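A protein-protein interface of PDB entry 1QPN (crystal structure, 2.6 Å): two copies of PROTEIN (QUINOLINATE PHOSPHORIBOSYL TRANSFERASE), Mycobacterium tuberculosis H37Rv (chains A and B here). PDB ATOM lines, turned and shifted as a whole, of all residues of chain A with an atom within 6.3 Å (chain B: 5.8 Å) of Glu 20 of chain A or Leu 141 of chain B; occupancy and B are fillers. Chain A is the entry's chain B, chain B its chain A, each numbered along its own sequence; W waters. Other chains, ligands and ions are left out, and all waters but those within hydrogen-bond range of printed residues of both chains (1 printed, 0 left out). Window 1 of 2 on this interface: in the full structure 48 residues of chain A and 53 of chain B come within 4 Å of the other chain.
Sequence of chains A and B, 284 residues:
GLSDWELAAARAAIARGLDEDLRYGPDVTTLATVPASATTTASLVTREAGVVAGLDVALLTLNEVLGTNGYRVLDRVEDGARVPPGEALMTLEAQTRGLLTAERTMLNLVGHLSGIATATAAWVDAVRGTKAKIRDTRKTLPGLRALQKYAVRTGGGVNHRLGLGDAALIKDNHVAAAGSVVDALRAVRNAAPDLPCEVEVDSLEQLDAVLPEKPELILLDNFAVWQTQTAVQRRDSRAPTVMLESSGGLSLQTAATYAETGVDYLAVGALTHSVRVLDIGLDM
N of Leu 164 of chain B is in hydrogen-bond range of O of Asp 21 of chain A (3.0 Å).
N of Leu 144 of chain B sits at hydrogen-bond distance from OE2 of Glu 20 of chain A (3.2 Å).
The side-chain carboxylate of Glu 20 of chain A is in hydrogen-bond range of the backbone NH of Gly 143 of chain B.
OE2 of Glu 20 of chain A is in hydrogen-bond range of N of Arg 145 of chain B, at 3.2 Å.
ND2 of Asn 108 of chain A lies within hydrogen-bond range of O of Thr 140 of chain B (3.1 Å).
NH1 of Arg 145 of chain B lies within salt-bridge range of OD1 of Asp 21 of chain A (3.1 Å).
O of Leu 162 of chain B is in hydrogen-bond range of NH1 of Arg 145 of chain B, at 2.5 Å.
The guanidinium group (NE) of Arg 145 of chain B is in hydrogen-bond range of the side-chain hydroxyl (OG1) of Thr 140 of chain B.
The backbone NH of Leu 141 of chain B lies close to the side-chain amide nitrogen of Gln 148 of chain B (2.9 Å).
The side-chain amide oxygen of Gln 148 of chain B is in hydrogen-bond range of a ring nitrogen (NE2) of His 112 of chain B (3.0 Å).
The backbone carbonyl oxygen (O) of Lys 139 of chain B is in hydrogen-bond range of the backbone NH (N) of His 273 of chain B, at 3.5 Å.
The side-chain hydroxyl (OG1) of Thr 272 of chain B is in hydrogen-bond range of the backbone carbonyl oxygen (O) of Lys 139 of chain B.
Leu 141 of chain B touches Glu 20 of chain A.
Pro 142 of chain B touches Glu 20 of chain A.
Leu 162 of chain B touches Glu 20 of chain A.
O of Asp 21 of chain A touches CA of Gly 163 of chain B (3.8 Å).
CE1 of Tyr 24 of chain A touches CB of Leu 162 of chain B, 3.8 Å away.
Lys 139 of chain B touches Asn 108 of chain A (CA to OD1, 3.6 Å).
Leu 109 of chain A touches Pro 142 of chain B.
Leu 141 of chain B touches His 112 of chain A (CD1 to ND1, 3.6 Å).
Leu 141 of chain A touches His 112 of chain B (CD1 to ND1, 3.5 Å).
Leu 141 of chain B touches just these residues of chain A: Glu 20 (3.9 Å) and His 112 (3.6 Å).
Printed residues of chain A within 4 Å of Leu 144 of chain B: Glu 20.
Of the printed residues of chain B, Leu 109 of chain A touches Pro 142.
Of the printed residues of chain B, Asn 108 of chain A touches Lys 139 and Thr 140.
Printed residues of chain A within 4 Å of Leu 164 of chain B: Asp 21 (3.0 Å).
Of the printed residues of chain B, Leu 141 of chain A touches His 112.
Leu 144 of chain A touches none of the printed residues of chain B.
Arg 23 of chain A touches none of the printed residues of chain B.
The nearest residue of chain A that does not touch Leu 141 of chain B is Leu 144 of chain A (4.1 Å).
The nearest printed residue of chain A that does not touch Leu 162 of chain B is Asp 21 of chain A (4.9 Å).
Of the 16 printed residues of chain B, 11 touch a printed residue of chain A.
Of the 15 printed residues of chain A, 7 touch a printed residue of chain B.
Hydrophobic or aromatic side chains of chain A that line the printed part of chain B: Tyr 24, Leu 109, His 112 and Leu 141.
Among the printed residues, 15 pairs touch across the chains.
Among the printed residues, Asp or Glu carboxylates within 4 Å of a Lys or Arg side-chain nitrogen of the other chain: Asp 21 of chain A with Arg 145 of chain B (3.1 Å).
His 112 of chain A touches Leu 141 of chain B, and with the chains exchanged Leu 141 of chain A touches His 112 of chain B.
Water W1 bridges the side-chain carboxylate (OE2) of Glu 20 of chain A (2.9 Å) and the backbone NH (N) of Ala 146 of chain B (3.0 Å).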
ATOM      1  N   ALA A  15      25.686  13.475  24.661  1.00  0.00           N
ATOM      2  CA  ALA A  15      26.464  14.492  23.989  1.00  0.00           C
ATOM      3  C   ALA A  15      26.667  14.107  22.524  1.00  0.00           C
ATOM      4  O   ALA A  15      26.465  14.945  21.637  1.00  0.00           O
ATOM      5  CB  ALA A  15      27.769  14.676  24.663  1.00  0.00           C
ATOM      6  N   ARG A  16      27.033  12.849  22.254  1.00  0.00           N
ATOM      7  CA  ARG A  16      27.245  12.376  20.881  1.00  0.00           C
ATOM      8  C   ARG A  16      25.968  12.519  20.077  1.00  0.00           C
ATOM      9  O   ARG A  16      25.989  12.916  18.903  1.00  0.00           O
ATOM     10  CB  ARG A  16      27.691  10.921  20.879  1.00  0.00           C
ATOM     11  CG  ARG A  16      29.061  10.673  21.482  1.00  0.00           C
ATOM     12  CD  ARG A  16      29.471   9.224  21.280  1.00  0.00           C
ATOM     13  NE  ARG A  16      28.971   8.309  22.314  1.00  0.00           N
ATOM     14  CZ  ARG A  16      29.667   7.966  23.402  1.00  0.00           C
ATOM     15  NH1 ARG A  16      30.895   8.462  23.591  1.00  0.00           N
ATOM     16  NH2 ARG A  16      29.134   7.134  24.304  1.00  0.00           N
ATOM     17  N   GLY A  17      24.846  12.239  20.729  1.00  0.00           N
ATOM     18  CA  GLY A  17      23.560  12.356  20.068  1.00  0.00           C
ATOM     19  C   GLY A  17      23.232  13.776  19.670  1.00  0.00           C
ATOM     20  O   GLY A  17      22.878  14.016  18.522  1.00  0.00           O
ATOM     21  N   LEU A  18      23.337  14.718  20.609  1.00  0.00           N
ATOM     22  CA  LEU A  18      23.060  16.123  20.319  1.00  0.00           C
ATOM     23  C   LEU A  18      23.985  16.641  19.281  1.00  0.00           C
ATOM     24  O   LEU A  18      23.583  17.475  18.491  1.00  0.00           O
ATOM     25  CB  LEU A  18      23.251  16.965  21.545  1.00  0.00           C
ATOM     26  CG  LEU A  18      22.176  16.706  22.553  1.00  0.00           C
ATOM     27  CD1 LEU A  18      22.575  17.405  23.797  1.00  0.00           C
ATOM     28  CD2 LEU A  18      20.894  17.246  21.973  1.00  0.00           C
ATOM     29  N   ASP A  19      25.233  16.171  19.290  1.00  0.00           N
ATOM     30  CA  ASP A  19      26.199  16.634  18.316  1.00  0.00           C
ATOM     31  C   ASP A  19      25.837  16.156  16.925  1.00  0.00           C
ATOM     32  O   ASP A  19      26.078  16.849  15.968  1.00  0.00           O
ATOM     33  CB  ASP A  19      27.619  16.240  18.709  1.00  0.00           C
ATOM     34  CG  ASP A  19      28.657  16.644  17.650  1.00  0.00           C
ATOM     35  OD1 ASP A  19      28.768  17.865  17.353  1.00  0.00           O
ATOM     36  OD2 ASP A  19      29.375  15.744  17.124  1.00  0.00           O
ATOM     37  N   GLU A  20      25.217  14.996  16.791  1.00  0.00           N
ATOM     38  CA  GLU A  20      24.845  14.533  15.452  1.00  0.00           C
ATOM     39  C   GLU A  20      23.731  15.397  14.880  1.00  0.00           C
ATOM     40  O   GLU A  20      23.697  15.675  13.687  1.00  0.00           O
ATOM     41  CB  GLU A  20      24.394  13.078  15.491  1.00  0.00           C
ATOM     42  CG  GLU A  20      25.475  12.116  15.944  1.00  0.00           C
ATOM     43  CD  GLU A  20      24.968  10.694  16.227  1.00  0.00           C
ATOM     44  OE1 GLU A  20      23.879  10.522  16.842  1.00  0.00           O
ATOM     45  OE2 GLU A  20      25.691   9.740  15.862  1.00  0.00           O
ATOM     46  N   ASP A  21      22.826  15.813  15.761  1.00  0.00           N
ATOM     47  CA  ASP A  21      21.675  16.649  15.417  1.00  0.00           C
ATOM     48  C   ASP A  21      22.011  18.102  15.110  1.00  0.00           C
ATOM     49  O   ASP A  21      21.466  18.691  14.181  1.00  0.00           O
ATOM     50  CB  ASP A  21      20.663  16.623  16.565  1.00  0.00           C
ATOM     51  CG  ASP A  21      19.389  15.859  16.222  1.00  0.00           C
ATOM     52  OD1 ASP A  21      19.274  15.224  15.141  1.00  0.00           O
ATOM     53  OD2 ASP A  21      18.480  15.900  17.067  1.00  0.00           O
ATOM     54  N   LEU A  22      22.881  18.690  15.917  1.00  0.00           N
ATOM     55  CA  LEU A  22      23.275  20.083  15.749  1.00  0.00           C
ATOM     56  C   LEU A  22      24.429  20.334  14.805  1.00  0.00           C
ATOM     57  O   LEU A  22      24.632  21.450  14.375  1.00  0.00           O
ATOM     58  CB  LEU A  22      23.553  20.710  17.106  1.00  0.00           C
ATOM     59  CG  LEU A  22      22.319  20.580  18.003  1.00  0.00           C
ATOM     60  CD1 LEU A  22      22.655  20.924  19.425  1.00  0.00           C
ATOM     61  CD2 LEU A  22      21.186  21.460  17.498  1.00  0.00           C
ATOM     62  N   ARG A  23      25.162  19.301  14.442  1.00  0.00           N
ATOM     63  CA  ARG A  23      26.285  19.448  13.520  1.00  0.00           C
ATOM     64  C   ARG A  23      25.960  20.288  12.250  1.00  0.00           C
ATOM     65  O   ARG A  23      26.835  20.996  11.729  1.00  0.00           O
ATOM     66  CB  ARG A  23      26.770  18.045  13.084  1.00  0.00           C
ATOM     67  CG  ARG A  23      27.938  18.020  12.105  1.00  0.00           C
ATOM     68  CD  ARG A  23      28.198  16.638  11.512  1.00  0.00           C
ATOM     69  NE  ARG A  23      28.102  15.575  12.504  1.00  0.00           N
ATOM     70  CZ  ARG A  23      28.855  15.495  13.602  1.00  0.00           C
ATOM     71  NH1 ARG A  23      29.777  16.424  13.859  1.00  0.00           N
ATOM     72  NH2 ARG A  23      28.677  14.483  14.455  1.00  0.00           N
ATOM     73  N   TYR A  24      24.720  20.221  11.754  1.00  0.00           N
ATOM     74  CA  TYR A  24      24.374  20.926  10.518  1.00  0.00           C
ATOM     75  C   TYR A  24      23.698  22.240  10.742  1.00  0.00           C
ATOM     76  O   TYR A  24      23.217  22.857   9.797  1.00  0.00           O
ATOM     77  CB  TYR A  24      23.507  20.048   9.604  1.00  0.00           C
ATOM     78  CG  TYR A  24      24.119  18.702   9.402  1.00  0.00           C
ATOM     79  CD1 TYR A  24      23.943  17.702  10.358  1.00  0.00           C
ATOM     80  CD2 TYR A  24      24.998  18.466   8.347  1.00  0.00           C
ATOM     81  CE1 TYR A  24      24.640  16.503  10.287  1.00  0.00           C
ATOM     82  CE2 TYR A  24      25.707  17.270   8.256  1.00  0.00           C
ATOM     83  CZ  TYR A  24      25.531  16.285   9.237  1.00  0.00           C
ATOM     84  OH  TYR A  24      26.271  15.105   9.206  1.00  0.00           O
ATOM     85  N   ASN A 108      15.129   8.815  21.287  1.00  0.00           N
ATOM     86  CA  ASN A 108      15.957   7.752  20.755  1.00  0.00           C
ATOM     87  C   ASN A 108      16.576   6.934  21.898  1.00  0.00           C
ATOM     88  O   ASN A 108      16.497   5.705  21.922  1.00  0.00           O
ATOM     89  CB  ASN A 108      17.041   8.332  19.848  1.00  0.00           C
ATOM     90  CG  ASN A 108      16.490   8.764  18.513  1.00  0.00           C
ATOM     91  OD1 ASN A 108      15.325   8.509  18.197  1.00  0.00           O
ATOM     92  ND2 ASN A 108      17.331   9.365  17.691  1.00  0.00           N
ATOM     93  N   LEU A 109      17.133   7.619  22.881  1.00  0.00           N
ATOM     94  CA  LEU A 109      17.757   6.947  24.010  1.00  0.00           C
ATOM     95  C   LEU A 109      16.776   6.127  24.850  1.00  0.00           C
ATOM     96  O   LEU A 109      16.925   4.913  24.942  1.00  0.00           O
ATOM     97  CB  LEU A 109      18.486   7.967  24.888  1.00  0.00           C
ATOM     98  CG  LEU A 109      19.966   7.677  25.188  1.00  0.00           C
ATOM     99  CD1 LEU A 109      20.481   6.349  24.549  1.00  0.00           C
ATOM    100  CD2 LEU A 109      20.764   8.855  24.695  1.00  0.00           C
ATOM    101  N   HIS A 112      15.101   3.195  23.130  1.00  0.00           N
ATOM    102  CA  HIS A 112      16.024   2.089  23.022  1.00  0.00           C
ATOM    103  C   HIS A 112      16.112   1.398  24.362  1.00  0.00           C
ATOM    104  O   HIS A 112      15.819   0.204  24.451  1.00  0.00           O
ATOM    105  CB  HIS A 112      17.406   2.563  22.625  1.00  0.00           C
ATOM    106  CG  HIS A 112      18.389   1.452  22.408  1.00  0.00           C
ATOM    107  ND1 HIS A 112      18.375   0.659  21.280  1.00  0.00           N
ATOM    108  CD2 HIS A 112      19.406   0.992  23.177  1.00  0.00           C
ATOM    109  CE1 HIS A 112      19.332  -0.245  21.365  1.00  0.00           C
ATOM    110  NE2 HIS A 112      19.974  -0.065  22.504  1.00  0.00           N
ATOM    111  N   LEU A 141      26.200  -2.589  21.634  1.00  0.00           N
ATOM    112  CA  LEU A 141      26.538  -1.616  20.588  1.00  0.00           C
ATOM    113  C   LEU A 141      27.637  -0.764  21.171  1.00  0.00           C
ATOM    114  O   LEU A 141      27.583  -0.369  22.360  1.00  0.00           O
ATOM    115  CB  LEU A 141      25.358  -0.747  20.190  1.00  0.00           C
ATOM    116  CG  LEU A 141      24.460  -1.143  19.028  1.00  0.00           C
ATOM    117  CD1 LEU A 141      25.213  -1.942  18.009  1.00  0.00           C
ATOM    118  CD2 LEU A 141      23.307  -1.932  19.539  1.00  0.00           C
ATOM    119  N   LEU A 144      27.560   2.094  23.904  1.00  0.00           N
ATOM    120  CA  LEU A 144      26.334   2.007  24.691  1.00  0.00           C
ATOM    121  C   LEU A 144      26.342   0.923  25.729  1.00  0.00           C
ATOM    122  O   LEU A 144      25.417   0.823  26.550  1.00  0.00           O
ATOM    123  CB  LEU A 144      25.127   1.834  23.757  1.00  0.00           C
ATOM    124  CG  LEU A 144      24.857   3.022  22.843  1.00  0.00           C
ATOM    125  CD1 LEU A 144      23.879   2.615  21.783  1.00  0.00           C
ATOM    126  CD2 LEU A 144      24.397   4.248  23.643  1.00  0.00           C
ATOM    127  N   HIS B 112      25.756  -5.380  13.256  1.00  0.00           N
ATOM    128  CA  HIS B 112      24.737  -4.350  13.323  1.00  0.00           C
ATOM    129  C   HIS B 112      24.516  -3.705  11.954  1.00  0.00           C
ATOM    130  O   HIS B 112      23.405  -3.620  11.450  1.00  0.00           O
ATOM    131  CB  HIS B 112      25.159  -3.290  14.290  1.00  0.00           C
ATOM    132  CG  HIS B 112      24.140  -2.215  14.496  1.00  0.00           C
ATOM    133  ND1 HIS B 112      23.031  -2.392  15.292  1.00  0.00           N
ATOM    134  CD2 HIS B 112      24.082  -0.945  14.037  1.00  0.00           C
ATOM    135  CE1 HIS B 112      22.333  -1.270  15.316  1.00  0.00           C
ATOM    136  NE2 HIS B 112      22.948  -0.378  14.563  1.00  0.00           N
ATOM    137  N   LYS B 139      15.721   8.576  13.643  1.00  0.00           N
ATOM    138  CA  LYS B 139      15.523   7.665  14.754  1.00  0.00           C
ATOM    139  C   LYS B 139      16.702   6.683  14.736  1.00  0.00           C
ATOM    140  O   LYS B 139      16.548   5.495  14.461  1.00  0.00           O
ATOM    141  CB  LYS B 139      14.218   6.945  14.585  1.00  0.00           C
ATOM    142  CG  LYS B 139      13.070   7.853  14.279  1.00  0.00           C
ATOM    143  CD  LYS B 139      11.809   7.224  14.787  1.00  0.00           C
ATOM    144  CE  LYS B 139      10.596   8.002  14.315  1.00  0.00           C
ATOM    145  NZ  LYS B 139       9.356   7.550  14.989  1.00  0.00           N
ATOM    146  N   THR B 140      17.892   7.238  14.994  1.00  0.00           N
ATOM    147  CA  THR B 140      19.156   6.538  15.007  1.00  0.00           C
ATOM    148  C   THR B 140      19.742   6.397  16.430  1.00  0.00           C
ATOM    149  O   THR B 140      19.283   7.041  17.364  1.00  0.00           O
ATOM    150  CB  THR B 140      20.097   7.316  14.124  1.00  0.00           C
ATOM    151  OG1 THR B 140      20.049   8.697  14.493  1.00  0.00           O
ATOM    152  CG2 THR B 140      19.684   7.191  12.662  1.00  0.00           C
ATOM    153  N   LEU B 141      20.689   5.490  16.637  1.00  0.00           N
ATOM    154  CA  LEU B 141      21.276   5.352  17.970  1.00  0.00           C
ATOM    155  C   LEU B 141      22.356   6.412  18.095  1.00  0.00           C
ATOM    156  O   LEU B 141      23.079   6.686  17.155  1.00  0.00           O
ATOM    157  CB  LEU B 141      21.909   3.976  18.177  1.00  0.00           C
ATOM    158  CG  LEU B 141      21.090   2.861  18.803  1.00  0.00           C
ATOM    159  CD1 LEU B 141      20.049   3.485  19.725  1.00  0.00           C
ATOM    160  CD2 LEU B 141      20.420   2.044  17.719  1.00  0.00           C
ATOM    161  N   PRO B 142      22.486   7.020  19.266  1.00  0.00           N
ATOM    162  CA  PRO B 142      23.491   8.065  19.519  1.00  0.00           C
ATOM    163  C   PRO B 142      24.940   7.647  19.306  1.00  0.00           C
ATOM    164  O   PRO B 142      25.448   6.792  19.999  1.00  0.00           O
ATOM    165  CB  PRO B 142      23.238   8.448  20.967  1.00  0.00           C
ATOM    166  CG  PRO B 142      22.455   7.263  21.515  1.00  0.00           C
ATOM    167  CD  PRO B 142      21.586   6.856  20.417  1.00  0.00           C
ATOM    168  N   GLY B 143      25.605   8.300  18.366  1.00  0.00           N
ATOM    169  CA  GLY B 143      26.978   7.998  18.089  1.00  0.00           C
ATOM    170  C   GLY B 143      27.098   7.129  16.876  1.00  0.00           C
ATOM    171  O   GLY B 143      28.191   6.973  16.354  1.00  0.00           O
ATOM    172  N   LEU B 144      25.986   6.588  16.383  1.00  0.00           N
ATOM    173  CA  LEU B 144      26.050   5.688  15.227  1.00  0.00           C
ATOM    174  C   LEU B 144      25.310   6.131  13.977  1.00  0.00           C
ATOM    175  O   LEU B 144      25.333   5.424  12.962  1.00  0.00           O
ATOM    176  CB  LEU B 144      25.551   4.294  15.626  1.00  0.00           C
ATOM    177  CG  LEU B 144      26.352   3.561  16.707  1.00  0.00           C
ATOM    178  CD1 LEU B 144      25.572   2.406  17.270  1.00  0.00           C
ATOM    179  CD2 LEU B 144      27.641   3.086  16.099  1.00  0.00           C
ATOM    180  N   ARG B 145      24.654   7.286  14.031  1.00  0.00           N
ATOM    181  CA  ARG B 145      23.921   7.788  12.868  1.00  0.00           C
ATOM    182  C   ARG B 145      24.621   7.669  11.525  1.00  0.00           C
ATOM    183  O   ARG B 145      24.055   7.079  10.607  1.00  0.00           O
ATOM    184  CB  ARG B 145      23.429   9.223  13.058  1.00  0.00           C
ATOM    185  CG  ARG B 145      22.807   9.781  11.778  1.00  0.00           C
ATOM    186  CD  ARG B 145      22.056  11.067  12.000  1.00  0.00           C
ATOM    187  NE  ARG B 145      21.053  10.918  13.033  1.00  0.00           N
ATOM    188  CZ  ARG B 145      20.515  11.935  13.683  1.00  0.00           C
ATOM    189  NH1 ARG B 145      20.889  13.174  13.390  1.00  0.00           N
ATOM    190  NH2 ARG B 145      19.654  11.718  14.670  1.00  0.00           N
ATOM    191  N   ALA B 146      25.838   8.200  11.396  1.00  0.00           N
ATOM    192  CA  ALA B 146      26.546   8.144  10.103  1.00  0.00           C
ATOM    193  C   ALA B 146      26.701   6.716   9.620  1.00  0.00           C
ATOM    194  O   ALA B 146      26.499   6.440   8.432  1.00  0.00           O
ATOM    195  CB  ALA B 146      27.908   8.824  10.180  1.00  0.00           C
ATOM    196  N   GLN B 148      24.828   3.988  10.588  1.00  0.00           N
ATOM    197  CA  GLN B 148      23.492   3.446  10.301  1.00  0.00           C
ATOM    198  C   GLN B 148      22.965   3.973   8.970  1.00  0.00           C
ATOM    199  O   GLN B 148      22.351   3.233   8.216  1.00  0.00           O
ATOM    200  CB  GLN B 148      22.502   3.777  11.415  1.00  0.00           C
ATOM    201  CG  GLN B 148      22.927   3.192  12.674  1.00  0.00           C
ATOM    202  CD  GLN B 148      21.873   3.263  13.722  1.00  0.00           C
ATOM    203  OE1 GLN B 148      21.570   2.273  14.372  1.00  0.00           O
ATOM    204  NE2 GLN B 148      21.357   4.446  13.962  1.00  0.00           N
ATOM    205  N   LEU B 162      20.060  14.189   7.994  1.00  0.00           N
ATOM    206  CA  LEU B 162      21.197  13.831   8.822  1.00  0.00           C
ATOM    207  C   LEU B 162      21.141  14.495  10.186  1.00  0.00           C
ATOM    208  O   LEU B 162      21.727  13.998  11.134  1.00  0.00           O
ATOM    209  CB  LEU B 162      22.509  14.176   8.124  1.00  0.00           C
ATOM    210  CG  LEU B 162      22.787  13.406   6.826  1.00  0.00           C
ATOM    211  CD1 LEU B 162      24.018  14.018   6.106  1.00  0.00           C
ATOM    212  CD2 LEU B 162      22.980  11.912   7.131  1.00  0.00           C
ATOM    213  N   GLY B 163      20.364  15.563  10.298  1.00  0.00           N
ATOM    214  CA  GLY B 163      20.259  16.274  11.541  1.00  0.00           C
ATOM    215  C   GLY B 163      19.226  17.349  11.417  1.00  0.00           C
ATOM    216  O   GLY B 163      18.653  17.525  10.351  1.00  0.00           O
ATOM    217  N   LEU B 164      19.064  18.113  12.491  1.00  0.00           N
ATOM    218  CA  LEU B 164      18.095  19.198  12.619  1.00  0.00           C
ATOM    219  C   LEU B 164      18.251  20.358  11.630  1.00  0.00           C
ATOM    220  O   LEU B 164      17.266  20.976  11.240  1.00  0.00           O
ATOM    221  CB  LEU B 164      18.210  19.757  14.023  1.00  0.00           C
ATOM    222  CG  LEU B 164      17.065  19.726  15.029  1.00  0.00           C
ATOM    223  CD1 LEU B 164      15.962  18.791  14.599  1.00  0.00           C
ATOM    224  CD2 LEU B 164      17.646  19.364  16.404  1.00  0.00           C
ATOM    225  N   THR B 272      16.624   1.609  11.464  1.00  0.00           N
ATOM    226  CA  THR B 272      17.692   2.059  12.362  1.00  0.00           C
ATOM    227  C   THR B 272      17.398   1.923  13.864  1.00  0.00           C
ATOM    228  O   THR B 272      18.321   1.782  14.677  1.00  0.00           O
ATOM    229  CB  THR B 272      18.159   3.490  11.963  1.00  0.00           C
ATOM    230  OG1 THR B 272      17.072   4.414  12.085  1.00  0.00           O
ATOM    231  CG2 THR B 272      18.615   3.498  10.514  1.00  0.00           C
ATOM    232  N   HIS B 273      16.152   2.073  14.268  1.00  0.00           N
ATOM    233  CA  HIS B 273      15.826   1.804  15.671  1.00  0.00           C
ATOM    234  C   HIS B 273      15.341   0.376  15.498  1.00  0.00           C
ATOM    235  O   HIS B 273      15.171  -0.055  14.387  1.00  0.00           O
ATOM    236  CB  HIS B 273      14.722   2.733  16.217  1.00  0.00           C
ATOM    237  CG  HIS B 273      13.373   2.594  15.565  1.00  0.00           C
ATOM    238  ND1 HIS B 273      12.554   1.500  15.751  1.00  0.00           N
ATOM    239  CD2 HIS B 273      12.636   3.489  14.863  1.00  0.00           C
ATOM    240  CE1 HIS B 273      11.371   1.731  15.212  1.00  0.00           C
ATOM    241  NE2 HIS B 273      11.394   2.933  14.667  1.00  0.00           N
ATOM    242  N   VAL B 275      16.770  -2.756  15.249  1.00  0.00           N
ATOM    243  CA  VAL B 275      17.500  -3.606  14.265  1.00  0.00           C
ATOM    244  C   VAL B 275      17.883  -4.981  14.851  1.00  0.00           C
ATOM    245  O   VAL B 275      18.299  -5.074  16.016  1.00  0.00           O
ATOM    246  CB  VAL B 275      18.803  -2.980  13.613  1.00  0.00           C
ATOM    247  CG1 VAL B 275      18.799  -1.484  13.632  1.00  0.00           C
ATOM    248  CG2 VAL B 275      20.035  -3.525  14.242  1.00  0.00           C
HETATM  249  O   HOH W   1      27.441   9.483  13.618  1.00  0.00           O
